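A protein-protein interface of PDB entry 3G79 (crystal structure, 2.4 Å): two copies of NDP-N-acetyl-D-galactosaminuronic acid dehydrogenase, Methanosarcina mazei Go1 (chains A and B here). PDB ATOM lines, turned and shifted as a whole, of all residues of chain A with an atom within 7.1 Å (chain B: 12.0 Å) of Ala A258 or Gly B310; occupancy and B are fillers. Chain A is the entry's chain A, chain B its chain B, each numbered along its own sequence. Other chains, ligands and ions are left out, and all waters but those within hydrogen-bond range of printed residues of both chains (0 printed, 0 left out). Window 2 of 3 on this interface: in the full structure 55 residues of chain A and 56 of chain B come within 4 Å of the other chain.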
ATOM      1  N   LEU A 252      35.049  22.716  16.460  1.00  0.00           N
ATOM      2  CA  LEU A 252      33.780  22.016  16.480  1.00  0.00           C
ATOM      3  C   LEU A 252      33.538  21.625  17.935  1.00  0.00           C
ATOM      4  O   LEU A 252      32.396  21.659  18.408  1.00  0.00           O
ATOM      5  CB  LEU A 252      33.814  20.792  15.574  1.00  0.00           C
ATOM      6  CG  LEU A 252      32.623  20.144  14.894  1.00  0.00           C
ATOM      7  CD1 LEU A 252      32.648  18.685  15.309  1.00  0.00           C
ATOM      8  CD2 LEU A 252      31.214  20.841  15.054  1.00  0.00           C
ATOM      9  N   ALA A 253      34.635  21.315  18.635  1.00  0.00           N
ATOM     10  CA  ALA A 253      34.573  21.033  20.053  1.00  0.00           C
ATOM     11  C   ALA A 253      33.946  22.216  20.816  1.00  0.00           C
ATOM     12  O   ALA A 253      32.998  22.010  21.550  1.00  0.00           O
ATOM     13  CB  ALA A 253      35.973  20.638  20.618  1.00  0.00           C
ATOM     14  N   LEU A 254      34.434  23.438  20.630  1.00  0.00           N
ATOM     15  CA  LEU A 254      33.746  24.594  21.230  1.00  0.00           C
ATOM     16  C   LEU A 254      32.239  24.625  20.865  1.00  0.00           C
ATOM     17  O   LEU A 254      31.422  24.703  21.725  1.00  0.00           O
ATOM     18  CB  LEU A 254      34.439  25.916  20.895  1.00  0.00           C
ATOM     19  CG  LEU A 254      35.932  25.901  21.175  1.00  0.00           C
ATOM     20  CD1 LEU A 254      36.633  27.101  20.604  1.00  0.00           C
ATOM     21  CD2 LEU A 254      36.168  25.834  22.646  1.00  0.00           C
ATOM     22  N   TYR A 255      31.884  24.459  19.599  1.00  0.00           N
ATOM     23  CA  TYR A 255      30.472  24.405  19.204  1.00  0.00           C
ATOM     24  C   TYR A 255      29.696  23.285  19.892  1.00  0.00           C
ATOM     25  O   TYR A 255      28.523  23.451  20.225  1.00  0.00           O
ATOM     26  CB  TYR A 255      30.357  24.296  17.680  1.00  0.00           C
ATOM     27  CG  TYR A 255      30.600  25.607  16.959  1.00  0.00           C
ATOM     28  CD1 TYR A 255      30.426  25.719  15.569  1.00  0.00           C
ATOM     29  CD2 TYR A 255      30.978  26.740  17.660  1.00  0.00           C
ATOM     30  CE1 TYR A 255      30.633  26.936  14.909  1.00  0.00           C
ATOM     31  CE2 TYR A 255      31.185  27.936  17.022  1.00  0.00           C
ATOM     32  CZ  TYR A 255      31.016  28.037  15.649  1.00  0.00           C
ATOM     33  OH  TYR A 255      31.231  29.273  15.058  1.00  0.00           O
ATOM     34  N   CYS A 256      30.358  22.145  20.141  1.00  0.00           N
ATOM     35  CA  CYS A 256      29.653  21.007  20.708  1.00  0.00           C
ATOM     36  C   CYS A 256      29.400  21.204  22.188  1.00  0.00           C
ATOM     37  O   CYS A 256      28.383  20.731  22.744  1.00  0.00           O
ATOM     38  CB  CYS A 256      30.395  19.703  20.466  1.00  0.00           C
ATOM     39  SG  CYS A 256      30.114  19.110  18.850  1.00  0.00           S
ATOM     40  N   GLU A 257      30.338  21.881  22.821  1.00  0.00           N
ATOM     41  CA  GLU A 257      30.128  22.324  24.177  1.00  0.00           C
ATOM     42  C   GLU A 257      28.883  23.195  24.294  1.00  0.00           C
ATOM     43  O   GLU A 257      28.048  22.974  25.165  1.00  0.00           O
ATOM     44  CB  GLU A 257      31.342  23.074  24.693  1.00  0.00           C
ATOM     45  CG  GLU A 257      32.346  22.199  25.310  1.00  0.00           C
ATOM     46  CD  GLU A 257      33.549  23.027  25.770  1.00  0.00           C
ATOM     47  OE1 GLU A 257      34.685  22.555  25.581  1.00  0.00           O
ATOM     48  OE2 GLU A 257      33.345  24.157  26.300  1.00  0.00           O
ATOM     49  N   ALA A 258      28.751  24.152  23.398  1.00  0.00           N
ATOM     50  CA  ALA A 258      27.612  25.057  23.438  1.00  0.00           C
ATOM     51  C   ALA A 258      26.284  24.315  23.268  1.00  0.00           C
ATOM     52  O   ALA A 258      25.282  24.772  23.786  1.00  0.00           O
ATOM     53  CB  ALA A 258      27.758  26.110  22.362  1.00  0.00           C
ATOM     54  N   MET A 259      26.274  23.192  22.540  1.00  0.00           N
ATOM     55  CA  MET A 259      25.018  22.535  22.155  1.00  0.00           C
ATOM     56  C   MET A 259      24.771  21.347  23.081  1.00  0.00           C
ATOM     57  O   MET A 259      23.814  20.594  22.915  1.00  0.00           O
ATOM     58  CB  MET A 259      24.986  22.124  20.646  1.00  0.00           C
ATOM     59  CG  MET A 259      24.641  23.262  19.648  1.00  0.00           C
ATOM     60  SD  MET A 259      24.689  22.913  17.842  1.00  0.00           S
ATOM     61  CE  MET A 259      26.469  23.060  17.766  1.00  0.00           C
ATOM     62  N   GLY A 260      25.628  21.176  24.077  1.00  0.00           N
ATOM     63  CA  GLY A 260      25.415  20.073  24.997  1.00  0.00           C
ATOM     64  C   GLY A 260      25.550  18.719  24.307  1.00  0.00           C
ATOM     65  O   GLY A 260      24.943  17.750  24.758  1.00  0.00           O
ATOM     66  N   ILE A 261      26.360  18.630  23.238  1.00  0.00           N
ATOM     67  CA  ILE A 261      26.563  17.333  22.537  1.00  0.00           C
ATOM     68  C   ILE A 261      28.025  16.827  22.535  1.00  0.00           C
ATOM     69  O   ILE A 261      28.938  17.593  22.737  1.00  0.00           O
ATOM     70  CB  ILE A 261      26.055  17.358  21.086  1.00  0.00           C
ATOM     71  CG1 ILE A 261      26.745  18.493  20.304  1.00  0.00           C
ATOM     72  CG2 ILE A 261      24.525  17.460  21.072  1.00  0.00           C
ATOM     73  CD1 ILE A 261      26.673  18.365  18.747  1.00  0.00           C
ATOM     74  N   GLU A 471      29.932  16.674  25.672  1.00  0.00           N
ATOM     75  CA  GLU A 471      28.447  16.958  25.629  1.00  0.00           C
ATOM     76  C   GLU A 471      28.217  18.288  26.290  1.00  0.00           C
ATOM     77  O   GLU A 471      28.905  19.247  25.952  1.00  0.00           O
ATOM     78  CB  GLU A 471      27.532  15.877  26.280  1.00  0.00           C
ATOM     79  CG  GLU A 471      27.586  14.437  25.791  1.00  0.00           C
ATOM     80  CD  GLU A 471      28.906  13.776  26.087  1.00  0.00           C
ATOM     81  OE1 GLU A 471      29.983  14.432  26.087  1.00  0.00           O
ATOM     82  OE2 GLU A 471      28.844  12.569  26.336  1.00  0.00           O
ATOM     83  N   HIS A 475      27.649  19.367  32.204  1.00  0.00           N
ATOM     84  CA  HIS A 475      26.573  19.914  32.978  1.00  0.00           C
ATOM     85  C   HIS A 475      25.967  18.779  33.782  1.00  0.00           C
ATOM     86  O   HIS A 475      24.835  18.869  34.256  1.00  0.00           O
ATOM     87  CB  HIS A 475      25.598  20.616  32.047  1.00  0.00           C
ATOM     88  CG  HIS A 475      26.011  22.016  31.701  1.00  0.00           C
ATOM     89  ND1 HIS A 475      27.320  22.450  31.775  1.00  0.00           N
ATOM     90  CD2 HIS A 475      25.285  23.087  31.283  1.00  0.00           C
ATOM     91  CE1 HIS A 475      27.385  23.723  31.419  1.00  0.00           C
ATOM     92  NE2 HIS A 475      26.162  24.134  31.111  1.00  0.00           N
ATOM     93  N   PRO B 151      20.192  21.822  12.891  1.00  0.00           N
ATOM     94  CA  PRO B 151      20.460  21.325  14.244  1.00  0.00           C
ATOM     95  C   PRO B 151      19.484  21.911  15.248  1.00  0.00           C
ATOM     96  O   PRO B 151      19.157  23.095  15.150  1.00  0.00           O
ATOM     97  CB  PRO B 151      21.885  21.803  14.543  1.00  0.00           C
ATOM     98  CG  PRO B 151      22.509  22.036  13.215  1.00  0.00           C
ATOM     99  CD  PRO B 151      21.412  22.309  12.222  1.00  0.00           C
ATOM    100  N   GLY B 152      19.017  21.092  16.186  1.00  0.00           N
ATOM    101  CA  GLY B 152      18.014  21.539  17.151  1.00  0.00           C
ATOM    102  C   GLY B 152      16.547  21.397  16.746  1.00  0.00           C
ATOM    103  O   GLY B 152      15.670  21.739  17.525  1.00  0.00           O
ATOM    104  N   GLU B 155      14.799  18.207  18.889  1.00  0.00           N
ATOM    105  CA  GLU B 155      14.507  18.681  20.255  1.00  0.00           C
ATOM    106  C   GLU B 155      13.667  19.965  20.303  1.00  0.00           C
ATOM    107  O   GLU B 155      13.135  20.289  21.343  1.00  0.00           O
ATOM    108  CB  GLU B 155      15.788  18.943  21.063  1.00  0.00           C
ATOM    109  CG  GLU B 155      16.788  17.799  21.116  1.00  0.00           C
ATOM    110  CD  GLU B 155      16.491  16.862  22.249  1.00  0.00           C
ATOM    111  OE1 GLU B 155      15.526  17.141  22.988  1.00  0.00           O
ATOM    112  OE2 GLU B 155      17.205  15.849  22.417  1.00  0.00           O
ATOM    113  N   SER B 227      23.136  11.068  19.975  1.00  0.00           N
ATOM    114  CA  SER B 227      21.962  11.850  20.341  1.00  0.00           C
ATOM    115  C   SER B 227      21.322  12.514  19.142  1.00  0.00           C
ATOM    116  O   SER B 227      21.961  12.683  18.098  1.00  0.00           O
ATOM    117  CB  SER B 227      22.368  12.913  21.363  1.00  0.00           C
ATOM    118  OG  SER B 227      22.867  14.042  20.707  1.00  0.00           O
ATOM    119  N   THR B 229      20.380  15.708  18.525  1.00  0.00           N
ATOM    120  CA  THR B 229      21.173  16.882  18.129  1.00  0.00           C
ATOM    121  C   THR B 229      22.553  16.506  17.514  1.00  0.00           C
ATOM    122  O   THR B 229      22.876  16.991  16.448  1.00  0.00           O
ATOM    123  CB  THR B 229      21.365  17.805  19.303  1.00  0.00           C
ATOM    124  OG1 THR B 229      20.158  17.820  20.056  1.00  0.00           O
ATOM    125  CG2 THR B 229      21.677  19.193  18.846  1.00  0.00           C
ATOM    126  N   ALA B 230      23.338  15.623  18.152  1.00  0.00           N
ATOM    127  CA  ALA B 230      24.647  15.190  17.592  1.00  0.00           C
ATOM    128  C   ALA B 230      24.520  14.664  16.148  1.00  0.00           C
ATOM    129  O   ALA B 230      25.387  14.919  15.316  1.00  0.00           O
ATOM    130  CB  ALA B 230      25.300  14.158  18.474  1.00  0.00           C
ATOM    131  N   GLU B 232      22.030  15.642  13.900  1.00  0.00           N
ATOM    132  CA  GLU B 232      21.817  16.784  13.002  1.00  0.00           C
ATOM    133  C   GLU B 232      23.104  17.593  12.804  1.00  0.00           C
ATOM    134  O   GLU B 232      23.373  18.096  11.713  1.00  0.00           O
ATOM    135  CB  GLU B 232      20.764  17.742  13.505  1.00  0.00           C
ATOM    136  CG  GLU B 232      19.336  17.229  13.758  1.00  0.00           C
ATOM    137  CD  GLU B 232      18.642  18.085  14.850  1.00  0.00           C
ATOM    138  OE1 GLU B 232      19.368  18.562  15.777  1.00  0.00           O
ATOM    139  OE2 GLU B 232      17.406  18.313  14.778  1.00  0.00           O
ATOM    140  N   VAL B 233      23.901  17.757  13.853  1.00  0.00           N
ATOM    141  CA  VAL B 233      25.167  18.464  13.723  1.00  0.00           C
ATOM    142  C   VAL B 233      26.213  17.714  12.824  1.00  0.00           C
ATOM    143  O   VAL B 233      27.023  18.348  12.110  1.00  0.00           O
ATOM    144  CB  VAL B 233      25.700  18.797  15.092  1.00  0.00           C
ATOM    145  CG1 VAL B 233      27.132  19.371  15.021  1.00  0.00           C
ATOM    146  CG2 VAL B 233      24.788  19.789  15.775  1.00  0.00           C
ATOM    147  N   HIS B 300      23.890  27.051   9.079  1.00  0.00           N
ATOM    148  CA  HIS B 300      22.946  26.279   9.900  1.00  0.00           C
ATOM    149  C   HIS B 300      23.581  25.781  11.201  1.00  0.00           C
ATOM    150  O   HIS B 300      22.953  25.800  12.264  1.00  0.00           O
ATOM    151  CB  HIS B 300      22.354  25.097   9.132  1.00  0.00           C
ATOM    152  CG  HIS B 300      21.682  25.483   7.849  1.00  0.00           C
ATOM    153  ND1 HIS B 300      21.628  24.645   6.747  1.00  0.00           N
ATOM    154  CD2 HIS B 300      21.034  26.620   7.490  1.00  0.00           C
ATOM    155  CE1 HIS B 300      20.986  25.253   5.766  1.00  0.00           C
ATOM    156  NE2 HIS B 300      20.619  26.453   6.187  1.00  0.00           N
ATOM    157  N   LEU B 301      24.828  25.353  11.108  1.00  0.00           N
ATOM    158  CA  LEU B 301      25.585  24.969  12.286  1.00  0.00           C
ATOM    159  C   LEU B 301      25.777  26.175  13.197  1.00  0.00           C
ATOM    160  O   LEU B 301      25.523  26.080  14.396  1.00  0.00           O
ATOM    161  CB  LEU B 301      26.914  24.277  11.923  1.00  0.00           C
ATOM    162  CG  LEU B 301      28.015  24.008  12.958  1.00  0.00           C
ATOM    163  CD1 LEU B 301      27.618  23.047  14.066  1.00  0.00           C
ATOM    164  CD2 LEU B 301      29.195  23.448  12.200  1.00  0.00           C
ATOM    165  N   GLU B 302      26.188  27.312  12.629  1.00  0.00           N
ATOM    166  CA  GLU B 302      26.287  28.523  13.429  1.00  0.00           C
ATOM    167  C   GLU B 302      24.909  29.003  13.987  1.00  0.00           C
ATOM    168  O   GLU B 302      24.838  29.397  15.161  1.00  0.00           O
ATOM    169  CB  GLU B 302      27.067  29.620  12.697  1.00  0.00           C
ATOM    170  CG  GLU B 302      28.414  29.122  12.173  1.00  0.00           C
ATOM    171  CD  GLU B 302      29.593  30.051  12.427  1.00  0.00           C
ATOM    172  OE1 GLU B 302      29.397  31.300  12.490  1.00  0.00           O
ATOM    173  OE2 GLU B 302      30.732  29.519  12.515  1.00  0.00           O
ATOM    174  N   ARG B 303      23.826  28.906  13.197  1.00  0.00           N
ATOM    175  CA  ARG B 303      22.494  29.315  13.691  1.00  0.00           C
ATOM    176  C   ARG B 303      22.123  28.403  14.833  1.00  0.00           C
ATOM    177  O   ARG B 303      21.588  28.851  15.840  1.00  0.00           O
ATOM    178  CB  ARG B 303      21.427  29.306  12.568  1.00  0.00           C
ATOM    179  CG  ARG B 303      19.965  29.112  13.001  1.00  0.00           C
ATOM    180  CD  ARG B 303      18.966  29.038  11.800  1.00  0.00           C
ATOM    181  NE  ARG B 303      18.453  30.361  11.400  1.00  0.00           N
ATOM    182  CZ  ARG B 303      19.106  31.209  10.597  1.00  0.00           C
ATOM    183  NH1 ARG B 303      20.296  30.875  10.103  1.00  0.00           N
ATOM    184  NH2 ARG B 303      18.590  32.402  10.303  1.00  0.00           N
ATOM    185  N   GLY B 304      22.452  27.128  14.662  1.00  0.00           N
ATOM    186  CA  GLY B 304      22.232  26.089  15.653  1.00  0.00           C
ATOM    187  C   GLY B 304      22.915  26.342  16.995  1.00  0.00           C
ATOM    188  O   GLY B 304      22.339  26.041  18.056  1.00  0.00           O
ATOM    189  N   VAL B 305      24.136  26.885  16.954  1.00  0.00           N
ATOM    190  CA  VAL B 305      24.837  27.246  18.166  1.00  0.00           C
ATOM    191  C   VAL B 305      24.043  28.361  18.817  1.00  0.00           C
ATOM    192  O   VAL B 305      23.722  28.304  20.006  1.00  0.00           O
ATOM    193  CB  VAL B 305      26.290  27.698  17.876  1.00  0.00           C
ATOM    194  CG1 VAL B 305      26.914  28.379  19.095  1.00  0.00           C
ATOM    195  CG2 VAL B 305      27.131  26.521  17.400  1.00  0.00           C
ATOM    196  N   LYS B 306      23.711  29.374  18.026  1.00  0.00           N
ATOM    197  CA  LYS B 306      22.900  30.486  18.516  1.00  0.00           C
ATOM    198  C   LYS B 306      21.539  30.081  19.054  1.00  0.00           C
ATOM    199  O   LYS B 306      21.198  30.434  20.164  1.00  0.00           O
ATOM    200  CB  LYS B 306      22.741  31.564  17.449  1.00  0.00           C
ATOM    201  CG  LYS B 306      23.858  32.553  17.517  1.00  0.00           C
ATOM    202  CD  LYS B 306      23.381  33.973  17.433  1.00  0.00           C
ATOM    203  CE  LYS B 306      22.508  34.385  18.585  1.00  0.00           C
ATOM    204  NZ  LYS B 306      22.106  35.810  18.330  1.00  0.00           N
ATOM    205  N   ILE B 307      20.749  29.344  18.277  1.00  0.00           N
ATOM    206  CA  ILE B 307      19.359  29.096  18.709  1.00  0.00           C
ATOM    207  C   ILE B 307      19.227  28.485  20.099  1.00  0.00           C
ATOM    208  O   ILE B 307      18.323  28.847  20.830  1.00  0.00           O
ATOM    209  CB  ILE B 307      18.564  28.272  17.708  1.00  0.00           C
ATOM    210  CG1 ILE B 307      18.069  29.155  16.567  1.00  0.00           C
ATOM    211  CG2 ILE B 307      17.371  27.635  18.391  1.00  0.00           C
ATOM    212  CD1 ILE B 307      17.378  28.376  15.450  1.00  0.00           C
ATOM    213  N   GLY B 308      20.147  27.591  20.472  1.00  0.00           N
ATOM    214  CA  GLY B 308      20.069  26.840  21.733  1.00  0.00           C
ATOM    215  C   GLY B 308      20.693  27.559  22.903  1.00  0.00           C
ATOM    216  O   GLY B 308      20.747  27.044  24.021  1.00  0.00           O
ATOM    217  N   ARG B 309      21.163  28.771  22.636  1.00  0.00           N
ATOM    218  CA  ARG B 309      21.765  29.635  23.651  1.00  0.00           C
ATOM    219  C   ARG B 309      22.614  28.926  24.720  1.00  0.00           C
ATOM    220  O   ARG B 309      22.614  29.332  25.879  1.00  0.00           O
ATOM    221  CB  ARG B 309      20.721  30.588  24.277  1.00  0.00           C
ATOM    222  CG  ARG B 309      19.277  30.108  24.219  1.00  0.00           C
ATOM    223  CD  ARG B 309      18.313  31.227  23.804  1.00  0.00           C
ATOM    224  NE  ARG B 309      18.780  31.972  22.622  1.00  0.00           N
ATOM    225  CZ  ARG B 309      17.987  32.549  21.720  1.00  0.00           C
ATOM    226  NH1 ARG B 309      16.668  32.482  21.829  1.00  0.00           N
ATOM    227  NH2 ARG B 309      18.519  33.200  20.699  1.00  0.00           N
ATOM    228  N   GLY B 310      23.351  27.881  24.331  1.00  0.00           N
ATOM    229  CA  GLY B 310      24.417  27.346  25.204  1.00  0.00           C
ATOM    230  C   GLY B 310      25.564  28.351  25.284  1.00  0.00           C
ATOM    231  O   GLY B 310      25.699  29.231  24.427  1.00  0.00           O
ATOM    232  N   GLU B 311      26.401  28.237  26.303  1.00  0.00           N
ATOM    233  CA  GLU B 311      27.490  29.201  26.470  1.00  0.00           C
ATOM    234  C   GLU B 311      28.721  28.880  25.582  1.00  0.00           C
ATOM    235  O   GLU B 311      29.370  27.832  25.768  1.00  0.00           O
ATOM    236  CB  GLU B 311      27.873  29.294  27.949  1.00  0.00           C
ATOM    237  CG  GLU B 311      28.507  30.623  28.372  1.00  0.00           C
ATOM    238  CD  GLU B 311      30.035  30.575  28.409  1.00  0.00           C
ATOM    239  OE1 GLU B 311      30.602  29.454  28.351  1.00  0.00           O
ATOM    240  OE2 GLU B 311      30.674  31.657  28.501  1.00  0.00           O
ATOM    241  N   LEU B 312      29.030  29.777  24.635  1.00  0.00           N
ATOM    242  CA  LEU B 312      30.183  29.623  23.740  1.00  0.00           C
ATOM    243  C   LEU B 312      31.301  30.549  24.169  1.00  0.00           C
ATOM    244  O   LEU B 312      31.069  31.743  24.292  1.00  0.00           O
ATOM    245  CB  LEU B 312      29.789  30.007  22.309  1.00  0.00           C
ATOM    246  CG  LEU B 312      30.027  29.206  21.008  1.00  0.00           C
ATOM    247  CD1 LEU B 312      30.247  30.195  19.867  1.00  0.00           C
ATOM    248  CD2 LEU B 312      31.149  28.207  20.996  1.00  0.00           C
ATOM    249  N   ASP B 313      32.492  30.008  24.442  1.00  0.00           N
ATOM    250  CA  ASP B 313      33.706  30.827  24.418  1.00  0.00           C
ATOM    251  C   ASP B 313      34.500  30.544  23.112  1.00  0.00           C
ATOM    252  O   ASP B 313      34.588  29.404  22.639  1.00  0.00           O
ATOM    253  CB  ASP B 313      34.544  30.794  25.737  1.00  0.00           C
ATOM    254  CG  ASP B 313      35.235  29.460  25.990  1.00  0.00           C
ATOM    255  OD1 ASP B 313      34.732  28.451  25.476  1.00  0.00           O
ATOM    256  OD2 ASP B 313      36.254  29.390  26.708  1.00  0.00           O
ATOM    257  N   TYR B 314      34.996  31.620  22.503  1.00  0.00           N
ATOM    258  CA  TYR B 314      35.696  31.601  21.224  1.00  0.00           C
ATOM    259  C   TYR B 314      36.530  32.860  21.330  1.00  0.00           C
ATOM    260  O   TYR B 314      36.143  33.773  22.092  1.00  0.00           O
ATOM    261  CB  TYR B 314      34.701  31.688  20.047  1.00  0.00           C
ATOM    262  CG  TYR B 314      35.286  31.309  18.672  1.00  0.00           C
ATOM    263  CD1 TYR B 314      35.695  29.989  18.392  1.00  0.00           C
ATOM    264  CD2 TYR B 314      35.428  32.260  17.650  1.00  0.00           C
ATOM    265  CE1 TYR B 314      36.248  29.628  17.117  1.00  0.00           C
ATOM    266  CE2 TYR B 314      35.979  31.911  16.389  1.00  0.00           C
ATOM    267  CZ  TYR B 314      36.373  30.590  16.123  1.00  0.00           C
ATOM    268  OH  TYR B 314      36.904  30.235  14.886  1.00  0.00           O
ATOM    269  N   GLU B 316      37.046  35.876  20.299  1.00  0.00           N
ATOM    270  CA  GLU B 316      36.364  37.140  20.599  1.00  0.00           C
ATOM    271  C   GLU B 316      34.891  37.250  20.094  1.00  0.00           C
ATOM    272  O   GLU B 316      34.014  36.503  20.573  1.00  0.00           O
ATOM    273  CB  GLU B 316      37.222  38.331  20.146  1.00  0.00           C
ATOM    274  CG  GLU B 316      37.894  39.072  21.319  1.00  0.00           C
ATOM    275  CD  GLU B 316      37.010  40.163  21.930  1.00  0.00           C
ATOM    276  OE1 GLU B 316      35.769  40.037  21.890  1.00  0.00           O
ATOM    277  OE2 GLU B 316      37.560  41.152  22.457  1.00  0.00           O
ATOM    278  N   TYR B 322      34.883  28.914   9.546  1.00  0.00           N
ATOM    279  CA  TYR B 322      33.954  28.296   8.624  1.00  0.00           C
ATOM    280  C   TYR B 322      33.362  29.421   7.797  1.00  0.00           C
ATOM    281  O   TYR B 322      33.332  29.367   6.588  1.00  0.00           O
ATOM    282  CB  TYR B 322      32.857  27.548   9.361  1.00  0.00           C
ATOM    283  CG  TYR B 322      33.297  26.533  10.392  1.00  0.00           C
ATOM    284  CD1 TYR B 322      34.469  25.780  10.218  1.00  0.00           C
ATOM    285  CD2 TYR B 322      32.487  26.242  11.504  1.00  0.00           C
ATOM    286  CE1 TYR B 322      34.876  24.786  11.172  1.00  0.00           C
ATOM    287  CE2 TYR B 322      32.865  25.233  12.447  1.00  0.00           C
ATOM    288  CZ  TYR B 322      34.075  24.522  12.264  1.00  0.00           C
ATOM    289  OH  TYR B 322      34.479  23.563  13.155  1.00  0.00           O
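OE2 of Glu B302 sits at hydrogen-bond distance from OH of Tyr A255, at 2.6 Å.
N of Leu A252 lies within hydrogen-bond range of OH of Tyr B322 (3.5 Å).
Among the printed residues, pairs that only touch across the chains: Leu A254 with Leu B312 (3.6 Å), Leu A254 with Asp B313 (3.7 Å), Leu A254 with Tyr B314 (3.8 Å), Tyr A255 with Leu B301 (3.9 Å), Tyr A255 with Val B305 (3.6 Å), Tyr A255 with Leu B312 (3.6 Å), Tyr A255 with Tyr B322 (3.7 Å), Ala A258 with Gly B310 (3.1 Å), Met A259 with Val B233 (3.7 Å), Met A259 with Leu B301 (3.9 Å), Met A259 with Gly B304 (3.9 Å), Met A259 with Val B305 (3.5 Å), Ile A261 with Ser B227 (3.8 Å), Ile A261 with Thr B229 (3.6 Å), Ile A261 with Ala B230 (3.6 Å) and Ile A261 with Val B233 (3.8 Å).
The backbone carbonyl oxygen (O) of Cys A256 sits at hydrogen-bond distance from the backbone NH (N) of Ile A261.
The side-chain hydroxyl (OG) of Ser B227 sits at hydrogen-bond distance from the backbone NH (N) of Ala B230, at 3.0 Å.
N of Glu A471 sits close to O of Ile A261 (3.2 Å).
The backbone carbonyl oxygen (O) of Leu A252 is in hydrogen-bond range of the side-chain sulfur (SG) of Cys A256.
Ala A258 touches one residue of chain B.
Gly B310 touches one residue of chain A.
No residue of chain B comes within 4 Å of Cys A256.
No residue of chain B comes within 4 Å of Glu A257.
No residue of chain B comes within 4 Å of Gly A260.
Printed residues of chain B within 4 Å of Leu A252: Tyr B322.
Printed residues of chain A within 4 Å of Thr B229: Ile A261.
Hydrophobic or aromatic side chains of chain A within 4 Å of the printed part of chain B: Leu A252, Leu A254, Tyr A255, Met A259 and Ile A261.
Along chain A the printed residues that touch a printed residue of chain B span positions 252 to 261.
Hydrophobic or aromatic side chains of chain B within 4 Å of the printed part of chain A: Val B233, Leu B301, Val B305, Leu B312, Tyr B314 and Tyr B322.
No position is printed for both chains.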
